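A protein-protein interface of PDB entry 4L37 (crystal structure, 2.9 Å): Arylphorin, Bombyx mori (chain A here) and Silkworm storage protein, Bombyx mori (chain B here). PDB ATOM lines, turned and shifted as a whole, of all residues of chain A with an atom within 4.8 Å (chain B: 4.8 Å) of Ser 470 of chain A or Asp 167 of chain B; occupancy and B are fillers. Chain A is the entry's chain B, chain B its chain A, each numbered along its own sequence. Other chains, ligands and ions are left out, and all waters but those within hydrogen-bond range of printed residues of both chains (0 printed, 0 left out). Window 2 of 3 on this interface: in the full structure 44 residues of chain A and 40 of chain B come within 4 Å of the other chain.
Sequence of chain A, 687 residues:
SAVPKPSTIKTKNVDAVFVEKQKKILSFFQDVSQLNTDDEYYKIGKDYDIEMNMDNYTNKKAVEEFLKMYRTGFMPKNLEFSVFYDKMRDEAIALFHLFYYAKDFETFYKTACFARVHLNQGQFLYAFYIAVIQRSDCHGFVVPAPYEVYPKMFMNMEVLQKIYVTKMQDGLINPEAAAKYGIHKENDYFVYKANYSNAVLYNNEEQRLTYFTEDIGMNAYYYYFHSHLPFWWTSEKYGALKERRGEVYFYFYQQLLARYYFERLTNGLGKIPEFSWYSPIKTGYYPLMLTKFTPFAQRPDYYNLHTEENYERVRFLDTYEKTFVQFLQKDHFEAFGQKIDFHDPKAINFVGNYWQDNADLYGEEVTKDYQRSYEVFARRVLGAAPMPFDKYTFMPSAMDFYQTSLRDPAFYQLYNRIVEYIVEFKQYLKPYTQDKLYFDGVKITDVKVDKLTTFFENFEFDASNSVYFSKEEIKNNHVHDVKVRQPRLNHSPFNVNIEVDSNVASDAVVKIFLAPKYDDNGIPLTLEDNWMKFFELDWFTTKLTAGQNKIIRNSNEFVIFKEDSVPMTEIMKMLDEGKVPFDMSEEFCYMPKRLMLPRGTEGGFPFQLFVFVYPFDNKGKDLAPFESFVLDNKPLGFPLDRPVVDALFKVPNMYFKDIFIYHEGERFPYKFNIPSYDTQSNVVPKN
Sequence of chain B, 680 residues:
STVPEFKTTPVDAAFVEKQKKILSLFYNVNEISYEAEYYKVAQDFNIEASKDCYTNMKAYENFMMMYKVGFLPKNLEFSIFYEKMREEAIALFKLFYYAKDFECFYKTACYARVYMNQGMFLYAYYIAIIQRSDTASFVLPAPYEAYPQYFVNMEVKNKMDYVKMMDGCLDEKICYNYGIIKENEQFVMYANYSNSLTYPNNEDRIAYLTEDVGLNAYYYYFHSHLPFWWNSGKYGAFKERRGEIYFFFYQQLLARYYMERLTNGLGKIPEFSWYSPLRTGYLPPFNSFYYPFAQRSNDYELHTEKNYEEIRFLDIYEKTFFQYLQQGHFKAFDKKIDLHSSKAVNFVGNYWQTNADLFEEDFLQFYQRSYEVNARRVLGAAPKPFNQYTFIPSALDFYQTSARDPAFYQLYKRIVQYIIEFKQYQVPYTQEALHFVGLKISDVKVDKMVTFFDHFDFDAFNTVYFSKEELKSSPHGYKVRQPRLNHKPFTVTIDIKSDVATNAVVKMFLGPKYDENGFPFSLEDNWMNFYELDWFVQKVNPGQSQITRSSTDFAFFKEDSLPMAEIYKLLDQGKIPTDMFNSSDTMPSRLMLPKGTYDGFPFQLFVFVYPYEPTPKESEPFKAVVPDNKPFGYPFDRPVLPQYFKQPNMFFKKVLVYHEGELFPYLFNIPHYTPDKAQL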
ATOM      1  N   TYR A 468      23.403 -24.795  -4.355  1.00  0.00           N
ATOM      2  CA  TYR A 468      22.422 -24.378  -3.374  1.00  0.00           C
ATOM      3  C   TYR A 468      21.322 -23.523  -4.001  1.00  0.00           C
ATOM      4  O   TYR A 468      21.607 -22.627  -4.790  1.00  0.00           O
ATOM      5  CB  TYR A 468      23.097 -23.621  -2.238  1.00  0.00           C
ATOM      6  CG  TYR A 468      24.029 -24.469  -1.430  1.00  0.00           C
ATOM      7  CD1 TYR A 468      23.892 -24.559  -0.045  1.00  0.00           C
ATOM      8  CD2 TYR A 468      25.066 -25.171  -2.046  1.00  0.00           C
ATOM      9  CE1 TYR A 468      24.759 -25.334   0.703  1.00  0.00           C
ATOM     10  CE2 TYR A 468      25.940 -25.952  -1.317  1.00  0.00           C
ATOM     11  CZ  TYR A 468      25.783 -26.034   0.056  1.00  0.00           C
ATOM     12  OH  TYR A 468      26.657 -26.825   0.771  1.00  0.00           O
ATOM     13  N   PHE A 469      20.065 -23.788  -3.609  1.00  0.00           N
ATOM     14  CA  PHE A 469      18.847 -23.163  -4.168  1.00  0.00           C
ATOM     15  C   PHE A 469      18.077 -22.335  -3.154  1.00  0.00           C
ATOM     16  O   PHE A 469      18.404 -22.306  -1.977  1.00  0.00           O
ATOM     17  CB  PHE A 469      17.938 -24.249  -4.719  1.00  0.00           C
ATOM     18  CG  PHE A 469      18.511 -24.987  -5.894  1.00  0.00           C
ATOM     19  CD1 PHE A 469      19.509 -25.939  -5.724  1.00  0.00           C
ATOM     20  CD2 PHE A 469      18.042 -24.737  -7.182  1.00  0.00           C
ATOM     21  CE1 PHE A 469      20.049 -26.632  -6.812  1.00  0.00           C
ATOM     22  CE2 PHE A 469      18.572 -25.423  -8.274  1.00  0.00           C
ATOM     23  CZ  PHE A 469      19.581 -26.380  -8.089  1.00  0.00           C
ATOM     24  N   SER A 470      17.035 -21.665  -3.608  1.00  0.00           N
ATOM     25  CA  SER A 470      16.287 -20.772  -2.733  1.00  0.00           C
ATOM     26  C   SER A 470      14.967 -21.362  -2.254  1.00  0.00           C
ATOM     27  O   SER A 470      14.365 -22.190  -2.954  1.00  0.00           O
ATOM     28  CB  SER A 470      15.991 -19.487  -3.470  1.00  0.00           C
ATOM     29  OG  SER A 470      15.629 -18.520  -2.530  1.00  0.00           O
ATOM     30  N   LYS A 471      14.505 -20.912  -1.076  1.00  0.00           N
ATOM     31  CA  LYS A 471      13.176 -21.276  -0.559  1.00  0.00           C
ATOM     32  C   LYS A 471      12.181 -21.210  -1.709  1.00  0.00           C
ATOM     33  O   LYS A 471      11.598 -22.228  -2.111  1.00  0.00           O
ATOM     34  CB  LYS A 471      12.740 -20.341   0.588  1.00  0.00           C
ATOM     35  CG  LYS A 471      11.616 -20.881   1.487  1.00  0.00           C
ATOM     36  CD  LYS A 471      12.038 -22.135   2.265  1.00  0.00           C
ATOM     37  CE  LYS A 471      10.936 -23.201   2.339  1.00  0.00           C
ATOM     38  NZ  LYS A 471       9.823 -22.825   3.265  1.00  0.00           N
ATOM     39  N   GLU A 472      12.050 -20.010  -2.262  1.00  0.00           N
ATOM     40  CA  GLU A 472      11.247 -19.768  -3.440  1.00  0.00           C
ATOM     41  C   GLU A 472      11.610 -20.689  -4.637  1.00  0.00           C
ATOM     42  O   GLU A 472      10.727 -21.195  -5.317  1.00  0.00           O
ATOM     43  CB  GLU A 472      11.305 -18.269  -3.795  1.00  0.00           C
ATOM     44  CG  GLU A 472      10.142 -17.734  -4.642  1.00  0.00           C
ATOM     45  CD  GLU A 472      10.485 -17.595  -6.129  1.00  0.00           C
ATOM     46  OE1 GLU A 472      11.194 -16.623  -6.486  1.00  0.00           O
ATOM     47  OE2 GLU A 472      10.041 -18.444  -6.946  1.00  0.00           O
ATOM     48  N   GLU A 473      12.885 -20.937  -4.892  1.00  0.00           N
ATOM     49  CA  GLU A 473      13.229 -21.771  -6.047  1.00  0.00           C
ATOM     50  C   GLU A 473      12.926 -23.263  -5.855  1.00  0.00           C
ATOM     51  O   GLU A 473      12.831 -24.014  -6.831  1.00  0.00           O
ATOM     52  CB  GLU A 473      14.702 -21.609  -6.412  1.00  0.00           C
ATOM     53  CG  GLU A 473      15.183 -20.171  -6.499  1.00  0.00           C
ATOM     54  CD  GLU A 473      16.646 -20.077  -6.911  1.00  0.00           C
ATOM     55  OE1 GLU A 473      17.395 -21.092  -6.815  1.00  0.00           O
ATOM     56  OE2 GLU A 473      17.045 -18.974  -7.335  1.00  0.00           O
ATOM     57  N   ILE A 474      12.812 -23.693  -4.600  1.00  0.00           N
ATOM     58  CA  ILE A 474      12.690 -25.121  -4.298  1.00  0.00           C
ATOM     59  C   ILE A 474      11.248 -25.575  -4.490  1.00  0.00           C
ATOM     60  O   ILE A 474      10.994 -26.629  -5.104  1.00  0.00           O
ATOM     61  CB  ILE A 474      13.284 -25.494  -2.910  1.00  0.00           C
ATOM     62  CG1 ILE A 474      14.786 -25.793  -3.056  1.00  0.00           C
ATOM     63  CG2 ILE A 474      12.551 -26.673  -2.275  1.00  0.00           C
ATOM     64  CD1 ILE A 474      15.404 -26.635  -1.959  1.00  0.00           C
ATOM     65  N   VAL B 163      24.818 -17.919   0.850  1.00  0.00           N
ATOM     66  CA  VAL B 163      23.693 -16.967   1.053  1.00  0.00           C
ATOM     67  C   VAL B 163      23.208 -16.299  -0.252  1.00  0.00           C
ATOM     68  O   VAL B 163      22.005 -16.155  -0.473  1.00  0.00           O
ATOM     69  CB  VAL B 163      24.046 -15.882   2.109  1.00  0.00           C
ATOM     70  CG1 VAL B 163      23.117 -14.686   1.991  1.00  0.00           C
ATOM     71  CG2 VAL B 163      24.013 -16.463   3.502  1.00  0.00           C
ATOM     72  N   LYS B 164      24.147 -15.897  -1.105  1.00  0.00           N
ATOM     73  CA  LYS B 164      23.801 -15.329  -2.393  1.00  0.00           C
ATOM     74  C   LYS B 164      23.124 -16.392  -3.275  1.00  0.00           C
ATOM     75  O   LYS B 164      22.113 -16.100  -3.936  1.00  0.00           O
ATOM     76  CB  LYS B 164      25.033 -14.771  -3.101  1.00  0.00           C
ATOM     77  CG  LYS B 164      24.813 -13.412  -3.727  1.00  0.00           C
ATOM     78  CD  LYS B 164      23.925 -13.498  -4.949  1.00  0.00           C
ATOM     79  CE  LYS B 164      23.481 -12.126  -5.427  1.00  0.00           C
ATOM     80  NZ  LYS B 164      23.018 -12.204  -6.848  1.00  0.00           N
ATOM     81  N   MET B 165      23.664 -17.613  -3.288  1.00  0.00           N
ATOM     82  CA  MET B 165      23.051 -18.710  -4.069  1.00  0.00           C
ATOM     83  C   MET B 165      21.624 -19.042  -3.603  1.00  0.00           C
ATOM     84  O   MET B 165      20.804 -19.447  -4.398  1.00  0.00           O
ATOM     85  CB  MET B 165      23.906 -19.989  -4.034  1.00  0.00           C
ATOM     86  CG  MET B 165      25.127 -20.010  -4.931  1.00  0.00           C
ATOM     87  SD  MET B 165      26.138 -21.476  -4.634  1.00  0.00           S
ATOM     88  CE  MET B 165      25.387 -22.678  -5.712  1.00  0.00           C
ATOM     89  N   MET B 166      21.337 -18.882  -2.319  1.00  0.00           N
ATOM     90  CA  MET B 166      20.016 -19.167  -1.821  1.00  0.00           C
ATOM     91  C   MET B 166      19.191 -17.913  -1.781  1.00  0.00           C
ATOM     92  O   MET B 166      18.062 -17.962  -1.313  1.00  0.00           O
ATOM     93  CB  MET B 166      20.058 -19.718  -0.408  1.00  0.00           C
ATOM     94  CG  MET B 166      20.686 -21.078  -0.263  1.00  0.00           C
ATOM     95  SD  MET B 166      20.944 -21.313   1.493  1.00  0.00           S
ATOM     96  CE  MET B 166      21.777 -22.906   1.484  1.00  0.00           C
ATOM     97  N   ASP B 167      19.758 -16.793  -2.229  1.00  0.00           N
ATOM     98  CA  ASP B 167      19.046 -15.503  -2.267  1.00  0.00           C
ATOM     99  C   ASP B 167      18.444 -15.114  -0.902  1.00  0.00           C
ATOM    100  O   ASP B 167      17.420 -14.432  -0.807  1.00  0.00           O
ATOM    101  CB  ASP B 167      17.985 -15.500  -3.388  1.00  0.00           C
ATOM    102  CG  ASP B 167      17.496 -14.087  -3.756  1.00  0.00           C
ATOM    103  OD1 ASP B 167      17.961 -13.088  -3.155  1.00  0.00           O
ATOM    104  OD2 ASP B 167      16.634 -13.979  -4.658  1.00  0.00           O
ATOM    105  N   GLY B 168      19.112 -15.554   0.150  1.00  0.00           N
ATOM    106  CA  GLY B 168      18.710 -15.241   1.497  1.00  0.00           C
ATOM    107  C   GLY B 168      19.002 -16.459   2.322  1.00  0.00           C
ATOM    108  O   GLY B 168      19.891 -17.232   2.000  1.00  0.00           O
ATOM    109  N   CYS B 169      18.245 -16.649   3.388  1.00  0.00           N
ATOM    110  CA  CYS B 169      18.429 -17.848   4.178  1.00  0.00           C
ATOM    111  C   CYS B 169      17.363 -18.944   4.060  1.00  0.00           C
ATOM    112  O   CYS B 169      16.160 -18.679   3.985  1.00  0.00           O
ATOM    113  CB  CYS B 169      18.726 -17.503   5.621  1.00  0.00           C
ATOM    114  SG  CYS B 169      20.415 -17.990   6.024  1.00  0.00           S
ATOM    115  N   PHE B 187      22.578  -8.059   4.369  1.00  0.00           N
ATOM    116  CA  PHE B 187      23.080  -9.197   5.157  1.00  0.00           C
ATOM    117  C   PHE B 187      24.216  -8.808   6.089  1.00  0.00           C
ATOM    118  O   PHE B 187      25.015  -7.954   5.745  1.00  0.00           O
ATOM    119  CB  PHE B 187      23.547 -10.307   4.244  1.00  0.00           C
ATOM    120  CG  PHE B 187      22.440 -10.889   3.432  1.00  0.00           C
ATOM    121  CD1 PHE B 187      21.448 -11.674   4.041  1.00  0.00           C
ATOM    122  CD2 PHE B 187      22.339 -10.613   2.068  1.00  0.00           C
ATOM    123  CE1 PHE B 187      20.385 -12.184   3.297  1.00  0.00           C
ATOM    124  CE2 PHE B 187      21.284 -11.115   1.321  1.00  0.00           C
ATOM    125  CZ  PHE B 187      20.303 -11.901   1.934  1.00  0.00           C
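The side-chain carboxylate (OE1) of Glu 473 of chain A lies within hydrogen-bond range of the backbone NH (N) of Ser 470 of chain A (3.3 Å).
Of chain B, only Met 166 (2.8 Å) and Asp 167 (3.9 Å) come within 4 Å of Ser 470 of chain A.
Of chain A, only Ser 470 comes within 4 Å of Asp 167 of chain B.
Of the printed residues of chain A, Met 166 of chain B touches Tyr 468 (3.1 Å), Phe 469 (3.1 Å) and Ser 470 (2.8 Å).
Printed residues of chain A within 4 Å of Met 165 of chain B: Tyr 468.
Printed residues of chain B within 4 Å of Tyr 468 of chain A: Met 165 and Met 166.
Printed residues of chain B within 4 Å of Phe 469 of chain A: Met 166 (3.1 Å).
Val 163 of chain B touches none of the printed residues of chain A.
The nearest residue of chain B that does not touch Ser 470 of chain A is Met 165 of chain B (4.4 Å).
Among the printed residues, pairs that only touch across the chains: Tyr 468 of chain A with Met 166 of chain B, Phe 469 of chain A with Met 166 of chain B and Ser 470 of chain A with Asp 167 of chain B.
O of Met 166 of chain B is in hydrogen-bond range of OG of Ser 470 of chain A (2.8 Å).
The backbone carbonyl oxygen of Tyr 468 of chain A sits close to the backbone carbonyl oxygen of Met 165 of chain B (3.3 Å).
Of the 7 printed residues of chain A, 3 touch a printed residue of chain B.
Hydrophobic or aromatic side chains of chain A that line the printed part of chain B: Tyr 468.
Along chain A the printed residues that touch a printed residue of chain B span positions 468 to 470.
Printed residues of chain B that touch a printed residue of chain A: Met 165, Met 166 and Asp 167.
Hydrophobic or aromatic side chains of chain B within 4 Å of the printed part of chain A: Met 165 and Met 166.
Along chain B the printed residues that touch a printed residue of chain A span positions 165 to 167.
Among the printed residues, 5 pairs touch across the chains.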
